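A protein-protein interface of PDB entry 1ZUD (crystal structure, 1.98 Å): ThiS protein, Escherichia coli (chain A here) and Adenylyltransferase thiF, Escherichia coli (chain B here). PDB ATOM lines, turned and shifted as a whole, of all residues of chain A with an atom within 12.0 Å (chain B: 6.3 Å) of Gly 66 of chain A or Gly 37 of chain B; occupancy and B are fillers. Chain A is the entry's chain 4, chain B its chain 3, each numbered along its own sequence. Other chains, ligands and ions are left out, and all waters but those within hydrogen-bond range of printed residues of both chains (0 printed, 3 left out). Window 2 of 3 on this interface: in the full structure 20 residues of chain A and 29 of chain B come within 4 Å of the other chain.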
ATOM      1  N   VAL A  62     -17.937 -18.091 -14.565  1.00  0.00           N
ATOM      2  CA  VAL A  62     -17.147 -19.136 -13.950  1.00  0.00           C
ATOM      3  C   VAL A  62     -17.328 -19.094 -12.399  1.00  0.00           C
ATOM      4  O   VAL A  62     -17.490 -18.010 -11.802  1.00  0.00           O
ATOM      5  CB  VAL A  62     -15.629 -18.946 -14.263  1.00  0.00           C
ATOM      6  CG1 VAL A  62     -15.117 -17.517 -13.742  1.00  0.00           C
ATOM      7  CG2 VAL A  62     -14.813 -20.162 -13.646  1.00  0.00           C
ATOM      8  N   ILE A  63     -17.331 -20.266 -11.759  1.00  0.00           N
ATOM      9  CA  ILE A  63     -17.366 -20.284 -10.290  1.00  0.00           C
ATOM     10  C   ILE A  63     -15.987 -20.885  -9.995  1.00  0.00           C
ATOM     11  O   ILE A  63     -15.637 -21.938 -10.518  1.00  0.00           O
ATOM     12  CB  ILE A  63     -18.454 -21.241  -9.713  1.00  0.00           C
ATOM     13  CG1 ILE A  63     -19.850 -20.707 -10.049  1.00  0.00           C
ATOM     14  CG2 ILE A  63     -18.213 -21.469  -8.177  1.00  0.00           C
ATOM     15  CD1 ILE A  63     -21.002 -21.687  -9.795  1.00  0.00           C
ATOM     16  N   ALA A  64     -15.218 -20.224  -9.151  1.00  0.00           N
ATOM     17  CA  ALA A  64     -13.895 -20.716  -8.798  1.00  0.00           C
ATOM     18  C   ALA A  64     -13.795 -21.182  -7.334  1.00  0.00           C
ATOM     19  O   ALA A  64     -12.848 -21.842  -6.995  1.00  0.00           O
ATOM     20  CB  ALA A  64     -12.879 -19.646  -9.057  1.00  0.00           C
ATOM     21  N   GLY A  65     -14.794 -20.911  -6.505  1.00  0.00           N
ATOM     22  CA  GLY A  65     -14.727 -21.323  -5.082  1.00  0.00           C
ATOM     23  C   GLY A  65     -14.781 -22.818  -4.783  1.00  0.00           C
ATOM     24  O   GLY A  65     -15.111 -23.595  -5.657  1.00  0.00           O
ATOM     25  N   GLY A  66     -14.503 -23.238  -3.549  1.00  0.00           N
ATOM     26  CA  GLY A  66     -14.496 -24.666  -3.259  1.00  0.00           C
ATOM     27  C   GLY A  66     -14.409 -25.038  -1.787  1.00  0.00           C
ATOM     28  O   GLY A  66     -13.763 -26.062  -1.394  1.00  0.00           O
ATOM     29  OXT GLY A  66     -15.046 -24.300  -1.016  1.00  0.00           O
ATOM     30  N   GLY B  35      -6.659 -29.312  -2.191  1.00  0.00           N
ATOM     31  CA  GLY B  35      -7.687 -28.509  -1.548  1.00  0.00           C
ATOM     32  C   GLY B  35      -8.475 -29.387  -0.589  1.00  0.00           C
ATOM     33  O   GLY B  35      -9.082 -30.350  -0.990  1.00  0.00           O
ATOM     34  N   LEU B  36      -8.412 -29.096   0.703  1.00  0.00           N
ATOM     35  CA  LEU B  36      -9.138 -29.900   1.694  1.00  0.00           C
ATOM     36  C   LEU B  36     -10.242 -29.067   2.357  1.00  0.00           C
ATOM     37  O   LEU B  36     -10.333 -28.956   3.606  1.00  0.00           O
ATOM     38  CB  LEU B  36      -8.156 -30.442   2.744  1.00  0.00           C
ATOM     39  CG  LEU B  36      -7.143 -31.438   2.150  1.00  0.00           C
ATOM     40  CD1 LEU B  36      -6.049 -31.862   3.194  1.00  0.00           C
ATOM     41  CD2 LEU B  36      -7.937 -32.647   1.626  1.00  0.00           C
ATOM     42  N   GLY B  37     -11.096 -28.514   1.495  1.00  0.00           N
ATOM     43  CA  GLY B  37     -12.195 -27.660   1.927  1.00  0.00           C
ATOM     44  C   GLY B  37     -13.556 -28.271   1.739  1.00  0.00           C
ATOM     45  O   GLY B  37     -13.742 -29.451   1.996  1.00  0.00           O
ATOM     46  N   GLY B  38     -14.530 -27.475   1.301  1.00  0.00           N
ATOM     47  CA  GLY B  38     -15.865 -28.026   1.114  1.00  0.00           C
ATOM     48  C   GLY B  38     -15.910 -29.124   0.039  1.00  0.00           C
ATOM     49  O   GLY B  38     -16.718 -30.086   0.080  1.00  0.00           O
ATOM     50  N   LEU B  39     -15.067 -28.994  -0.973  1.00  0.00           N
ATOM     51  CA  LEU B  39     -15.095 -30.009  -2.041  1.00  0.00           C
ATOM     52  C   LEU B  39     -14.221 -31.194  -1.636  1.00  0.00           C
ATOM     53  O   LEU B  39     -14.549 -32.376  -1.822  1.00  0.00           O
ATOM     54  CB  LEU B  39     -14.469 -29.436  -3.344  1.00  0.00           C
ATOM     55  CG  LEU B  39     -15.222 -28.294  -4.015  1.00  0.00           C
ATOM     56  CD1 LEU B  39     -14.348 -27.679  -5.166  1.00  0.00           C
ATOM     57  CD2 LEU B  39     -16.546 -28.908  -4.599  1.00  0.00           C
ATOM     58  N   GLY B  40     -13.055 -30.840  -1.137  1.00  0.00           N
ATOM     59  CA  GLY B  40     -12.086 -31.856  -0.831  1.00  0.00           C
ATOM     60  C   GLY B  40     -12.378 -32.765   0.337  1.00  0.00           C
ATOM     61  O   GLY B  40     -12.015 -33.953   0.260  1.00  0.00           O
ATOM     62  N   THR B  41     -12.987 -32.239   1.400  1.00  0.00           N
ATOM     63  CA  THR B  41     -13.208 -33.143   2.535  1.00  0.00           C
ATOM     64  C   THR B  41     -14.191 -34.294   2.194  1.00  0.00           C
ATOM     65  O   THR B  41     -13.880 -35.431   2.501  1.00  0.00           O
ATOM     66  CB  THR B  41     -13.660 -32.373   3.799  1.00  0.00           C
ATOM     67  OG1 THR B  41     -14.815 -31.595   3.512  1.00  0.00           O
ATOM     68  CG2 THR B  41     -12.553 -31.457   4.275  1.00  0.00           C
ATOM     69  N   PRO B  42     -15.359 -34.040   1.548  1.00  0.00           N
ATOM     70  CA  PRO B  42     -16.180 -35.243   1.264  1.00  0.00           C
ATOM     71  C   PRO B  42     -15.514 -36.121   0.213  1.00  0.00           C
ATOM     72  O   PRO B  42     -15.621 -37.357   0.284  1.00  0.00           O
ATOM     73  CB  PRO B  42     -17.502 -34.711   0.742  1.00  0.00           C
ATOM     74  CG  PRO B  42     -17.188 -33.308   0.347  1.00  0.00           C
ATOM     75  CD  PRO B  42     -16.054 -32.803   1.148  1.00  0.00           C
ATOM     76  N   ASP B  59      -3.015 -29.239   1.249  1.00  0.00           N
ATOM     77  CA  ASP B  59      -3.753 -28.018   1.600  1.00  0.00           C
ATOM     78  C   ASP B  59      -2.802 -27.173   2.453  1.00  0.00           C
ATOM     79  O   ASP B  59      -2.005 -27.720   3.204  1.00  0.00           O
ATOM     80  CB  ASP B  59      -5.043 -28.344   2.390  1.00  0.00           C
ATOM     81  CG  ASP B  59      -6.026 -27.118   2.513  1.00  0.00           C
ATOM     82  OD1 ASP B  59      -6.996 -26.965   1.703  1.00  0.00           O
ATOM     83  OD2 ASP B  59      -5.826 -26.294   3.438  1.00  0.00           O
ATOM     84  N   ARG B  70     -19.141 -26.604   6.494  1.00  0.00           N
ATOM     85  CA  ARG B  70     -19.131 -27.382   5.231  1.00  0.00           C
ATOM     86  C   ARG B  70     -18.003 -28.365   5.093  1.00  0.00           C
ATOM     87  O   ARG B  70     -18.007 -29.194   4.192  1.00  0.00           O
ATOM     88  CB  ARG B  70     -19.116 -26.414   4.006  1.00  0.00           C
ATOM     89  CG  ARG B  70     -17.881 -25.543   3.902  1.00  0.00           C
ATOM     90  CD  ARG B  70     -18.084 -24.298   3.031  1.00  0.00           C
ATOM     91  NE  ARG B  70     -16.917 -23.412   3.130  1.00  0.00           N
ATOM     92  CZ  ARG B  70     -16.611 -22.737   4.231  1.00  0.00           C
ATOM     93  NH1 ARG B  70     -17.405 -22.825   5.303  1.00  0.00           N
ATOM     94  NH2 ARG B  70     -15.484 -22.037   4.295  1.00  0.00           N
ATOM     95  N   GLN B  71     -17.000 -28.273   5.957  1.00  0.00           N
ATOM     96  CA  GLN B  71     -15.840 -29.172   5.853  1.00  0.00           C
ATOM     97  C   GLN B  71     -16.008 -30.242   6.921  1.00  0.00           C
ATOM     98  O   GLN B  71     -15.402 -30.151   8.007  1.00  0.00           O
ATOM     99  CB  GLN B  71     -14.583 -28.340   6.041  1.00  0.00           C
ATOM    100  CG  GLN B  71     -14.507 -27.264   4.884  1.00  0.00           C
ATOM    101  CD  GLN B  71     -13.380 -26.280   5.002  1.00  0.00           C
ATOM    102  OE1 GLN B  71     -12.381 -26.527   5.677  1.00  0.00           O
ATOM    103  NE2 GLN B  71     -13.500 -25.169   4.280  1.00  0.00           N
ATOM    104  N   ILE B  72     -16.825 -31.235   6.558  1.00  0.00           N
ATOM    105  CA  ILE B  72     -17.303 -32.355   7.382  1.00  0.00           C
ATOM    106  C   ILE B  72     -16.338 -33.358   7.954  1.00  0.00           C
ATOM    107  O   ILE B  72     -16.737 -34.227   8.740  1.00  0.00           O
ATOM    108  CB  ILE B  72     -18.392 -33.162   6.631  1.00  0.00           C
ATOM    109  CG1 ILE B  72     -17.761 -33.890   5.437  1.00  0.00           C
ATOM    110  CG2 ILE B  72     -19.525 -32.234   6.194  1.00  0.00           C
ATOM    111  CD1 ILE B  72     -18.756 -34.629   4.579  1.00  0.00           C
ATOM    112  N   PHE B  74     -13.649 -32.335   9.654  1.00  0.00           N
ATOM    113  CA  PHE B  74     -13.073 -31.677  10.830  1.00  0.00           C
ATOM    114  C   PHE B  74     -14.016 -31.490  12.036  1.00  0.00           C
ATOM    115  O   PHE B  74     -15.203 -31.621  11.900  1.00  0.00           O
ATOM    116  CB  PHE B  74     -12.533 -30.311  10.395  1.00  0.00           C
ATOM    117  CG  PHE B  74     -11.700 -30.375   9.142  1.00  0.00           C
ATOM    118  CD1 PHE B  74     -11.903 -29.490   8.112  1.00  0.00           C
ATOM    119  CD2 PHE B  74     -10.680 -31.334   9.024  1.00  0.00           C
ATOM    120  CE1 PHE B  74     -11.093 -29.551   6.957  1.00  0.00           C
ATOM    121  CE2 PHE B  74      -9.873 -31.401   7.897  1.00  0.00           C
ATOM    122  CZ  PHE B  74     -10.089 -30.499   6.861  1.00  0.00           C
ATOM    123  N   LYS B  83      -4.659 -28.473   8.190  1.00  0.00           N
ATOM    124  CA  LYS B  83      -5.675 -29.286   7.541  1.00  0.00           C
ATOM    125  C   LYS B  83      -5.227 -30.616   6.980  1.00  0.00           C
ATOM    126  O   LYS B  83      -5.949 -31.615   7.121  1.00  0.00           O
ATOM    127  CB  LYS B  83      -6.414 -28.501   6.447  1.00  0.00           C
ATOM    128  CG  LYS B  83      -7.540 -27.646   6.988  1.00  0.00           C
ATOM    129  CD  LYS B  83      -8.330 -26.977   5.866  1.00  0.00           C
ATOM    130  CE  LYS B  83      -9.172 -25.878   6.466  1.00  0.00           C
ATOM    131  NZ  LYS B  83      -9.925 -25.079   5.448  1.00  0.00           N
ATOM    132  N   CYS B 125      -9.775 -29.304  -6.062  1.00  0.00           N
ATOM    133  CA  CYS B 125     -10.764 -28.868  -5.091  1.00  0.00           C
ATOM    134  C   CYS B 125     -10.293 -27.549  -4.494  1.00  0.00           C
ATOM    135  O   CYS B 125     -10.487 -27.297  -3.298  1.00  0.00           O
ATOM    136  CB  CYS B 125     -10.868 -29.903  -3.996  1.00  0.00           C
ATOM    137  SG  CYS B 125     -11.306 -31.527  -4.565  1.00  0.00           S
ATOM    138  N   THR B 126      -9.663 -26.710  -5.317  1.00  0.00           N
ATOM    139  CA  THR B 126      -9.111 -25.443  -4.822  1.00  0.00           C
ATOM    140  C   THR B 126     -10.109 -24.288  -4.939  1.00  0.00           C
ATOM    141  O   THR B 126     -11.263 -24.497  -5.296  1.00  0.00           O
ATOM    142  CB  THR B 126      -7.731 -25.068  -5.515  1.00  0.00           C
ATOM    143  OG1 THR B 126      -7.909 -24.895  -6.938  1.00  0.00           O
ATOM    144  CG2 THR B 126      -6.708 -26.174  -5.259  1.00  0.00           C
ATOM    145  N   ASP B 127      -9.680 -23.072  -4.651  1.00  0.00           N
ATOM    146  CA  ASP B 127     -10.655 -21.992  -4.617  1.00  0.00           C
ATOM    147  C   ASP B 127     -10.245 -20.727  -5.357  1.00  0.00           C
ATOM    148  O   ASP B 127     -10.733 -19.646  -5.010  1.00  0.00           O
ATOM    149  CB  ASP B 127     -10.888 -21.587  -3.166  1.00  0.00           C
ATOM    150  CG  ASP B 127      -9.602 -21.067  -2.534  1.00  0.00           C
ATOM    151  OD1 ASP B 127      -9.574 -20.817  -1.315  1.00  0.00           O
ATOM    152  OD2 ASP B 127      -8.600 -20.904  -3.283  1.00  0.00           O
ATOM    153  N   ARG B 132      -6.073 -23.101 -10.142  1.00  0.00           N
ATOM    154  CA  ARG B 132      -6.748 -24.024 -11.014  1.00  0.00           C
ATOM    155  C   ARG B 132      -6.065 -24.025 -12.382  1.00  0.00           C
ATOM    156  O   ARG B 132      -5.891 -25.090 -12.974  1.00  0.00           O
ATOM    157  CB  ARG B 132      -8.241 -23.660 -11.158  1.00  0.00           C
ATOM    158  CG  ARG B 132      -9.111 -23.917  -9.869  1.00  0.00           C
ATOM    159  CD  ARG B 132     -10.522 -23.348 -10.037  1.00  0.00           C
ATOM    160  NE  ARG B 132     -11.378 -23.563  -8.866  1.00  0.00           N
ATOM    161  CZ  ARG B 132     -11.955 -24.733  -8.566  1.00  0.00           C
ATOM    162  NH1 ARG B 132     -11.778 -25.813  -9.336  1.00  0.00           N
ATOM    163  NH2 ARG B 132     -12.745 -24.825  -7.516  1.00  0.00           N
ATOM    164  N   ALA B 149     -14.027 -29.309  -9.878  1.00  0.00           N
ATOM    165  CA  ALA B 149     -15.372 -28.832  -9.504  1.00  0.00           C
ATOM    166  C   ALA B 149     -15.270 -27.542  -8.713  1.00  0.00           C
ATOM    167  O   ALA B 149     -14.219 -27.210  -8.229  1.00  0.00           O
ATOM    168  CB  ALA B 149     -16.112 -29.919  -8.679  1.00  0.00           C
ATOM    169  N   SER B 150     -16.377 -26.805  -8.618  1.00  0.00           N
ATOM    170  CA  SER B 150     -16.399 -25.566  -7.882  1.00  0.00           C
ATOM    171  C   SER B 150     -17.843 -25.360  -7.390  1.00  0.00           C
ATOM    172  O   SER B 150     -18.810 -26.024  -7.859  1.00  0.00           O
ATOM    173  CB  SER B 150     -15.984 -24.393  -8.801  1.00  0.00           C
ATOM    174  OG  SER B 150     -16.849 -24.348  -9.926  1.00  0.00           O
ATOM    175  N   ALA B 151     -17.998 -24.464  -6.422  1.00  0.00           N
ATOM    176  CA  ALA B 151     -19.340 -24.160  -5.940  1.00  0.00           C
ATOM    177  C   ALA B 151     -19.306 -22.831  -5.226  1.00  0.00           C
ATOM    178  O   ALA B 151     -18.281 -22.501  -4.652  1.00  0.00           O
ATOM    179  CB  ALA B 151     -19.825 -25.289  -4.964  1.00  0.00           C
ATOM    180  N   VAL B 152     -20.416 -22.087  -5.267  1.00  0.00           N
ATOM    181  CA  VAL B 152     -20.523 -20.812  -4.558  1.00  0.00           C
ATOM    182  C   VAL B 152     -22.014 -20.584  -4.442  1.00  0.00           C
ATOM    183  O   VAL B 152     -22.758 -20.942  -5.348  1.00  0.00           O
ATOM    184  CB  VAL B 152     -19.801 -19.586  -5.316  1.00  0.00           C
ATOM    185  CG1 VAL B 152     -20.566 -19.133  -6.551  1.00  0.00           C
ATOM    186  CG2 VAL B 152     -19.674 -18.392  -4.370  1.00  0.00           C
ATOM    187  N   VAL B 189     -21.754 -19.772   0.789  1.00  0.00           N
ATOM    188  CA  VAL B 189     -22.022 -21.043   0.163  1.00  0.00           C
ATOM    189  C   VAL B 189     -22.766 -21.964   1.127  1.00  0.00           C
ATOM    190  O   VAL B 189     -22.574 -21.935   2.375  1.00  0.00           O
ATOM    191  CB  VAL B 189     -20.709 -21.670  -0.328  1.00  0.00           C
ATOM    192  CG1 VAL B 189     -19.841 -22.053   0.861  1.00  0.00           C
ATOM    193  CG2 VAL B 189     -21.012 -22.865  -1.275  1.00  0.00           C
ATOM    194  N   VAL B 194     -21.725 -27.428  -1.963  1.00  0.00           N
ATOM    195  CA  VAL B 194     -20.319 -27.684  -2.252  1.00  0.00           C
ATOM    196  C   VAL B 194     -20.057 -29.176  -1.940  1.00  0.00           C
ATOM    197  O   VAL B 194     -19.241 -29.848  -2.590  1.00  0.00           O
ATOM    198  CB  VAL B 194     -19.340 -26.717  -1.460  1.00  0.00           C
ATOM    199  CG1 VAL B 194     -19.447 -26.902   0.067  1.00  0.00           C
ATOM    200  CG2 VAL B 194     -17.919 -27.050  -1.851  1.00  0.00           C
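Among the printed residues, merely in contact across the chains: Ile 63 of chain A with Ala 151 of chain B, Ile 63 of chain A with Val 152 of chain B, Ala 64 of chain A with Thr 126 of chain B, Ala 64 of chain A with Asp 127 of chain B, Gly 65 of chain A with Thr 126 of chain B, Gly 65 of chain A with Ser 150 of chain B, Gly 66 of chain A with Gly 37 of chain B, Gly 66 of chain A with Cys 125 of chain B, Gly 66 of chain A with Thr 126 of chain B and Gly 66 of chain A with Asp 127 of chain B.
Among the printed residues, 16 pairs touch across the chains. Among the printed residues, no Asp or Glu carboxylate lies within 4 Å of a Lys or Arg side-chain nitrogen of the other chain.
Of the printed residues of chain B, Gly 66 of chain A touches Gly 37 (3.8 Å), Gly 38 (3.1 Å), Leu 39 (3.2 Å), Cys 125 (3.99 Å), Thr 126 (3.8 Å) and Asp 127 (3.99 Å). Gly 37 of chain B touches just one residue of chain A: Gly 66. Gly 35 of chain B touches none of the printed residues of chain A. Of the printed residues of chain A, Leu 39 of chain B touches Gly 66. No residue of chain A comes within 4 Å of Gly 40 of chain B. No residue of chain A comes within 4 Å of Thr 41 of chain B. No residue of chain A comes within 4 Å of Arg 70 of chain B. Ser 150 of chain B touches just these residues of chain A: Ile 63 (2.8 Å) and Gly 65 (3.2 Å). No residue of chain A comes within 4 Å of Val 194 of chain B. Of the printed residues of chain A, Val 152 of chain B touches Ile 63. Of the printed residues of chain B, Ile 63 of chain A touches Ser 150 (2.8 Å), Ala 151 (3.4 Å) and Val 152 (3.7 Å). Of the printed residues of chain A, Ala 151 of chain B touches Ile 63 and Gly 65.
OG1 of Thr 41 of chain B is in hydrogen-bond range of O of Gly 37 of chain B, 2.8 Å away. The backbone carbonyl oxygen of Thr 126 of chain B lies within hydrogen-bond range of the guanidinium group of Arg 132 of chain B (2.7 Å). The backbone carbonyl oxygen of Ala 149 of chain B is in hydrogen-bond range of the guanidinium group of Arg 132 of chain B.
The backbone carbonyl oxygen (O) of Gly 65 of chain A is in hydrogen-bond range of the backbone NH (N) of Ala 151 of chain B (3.1 Å). The backbone carbonyl oxygen (O) of Ala 64 of chain A lies within hydrogen-bond range of the guanidinium group (NE) of Arg 132 of chain B (2.9 Å). The chain-end carboxylate (O) of Gly 66 of chain A sits at hydrogen-bond distance from the backbone NH (N) of Leu 39 of chain B (3.2 Å). N of Gly 38 of chain B sits at hydrogen-bond distance from O of Gly 66 of chain A (3.1 Å). OG of Ser 150 of chain B lies within hydrogen-bond range of O of Ile 63 of chain A, 2.8 Å away. O of Gly 65 of chain A sits at hydrogen-bond distance from NH2 of Arg 132 of chain B (3.3 Å).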
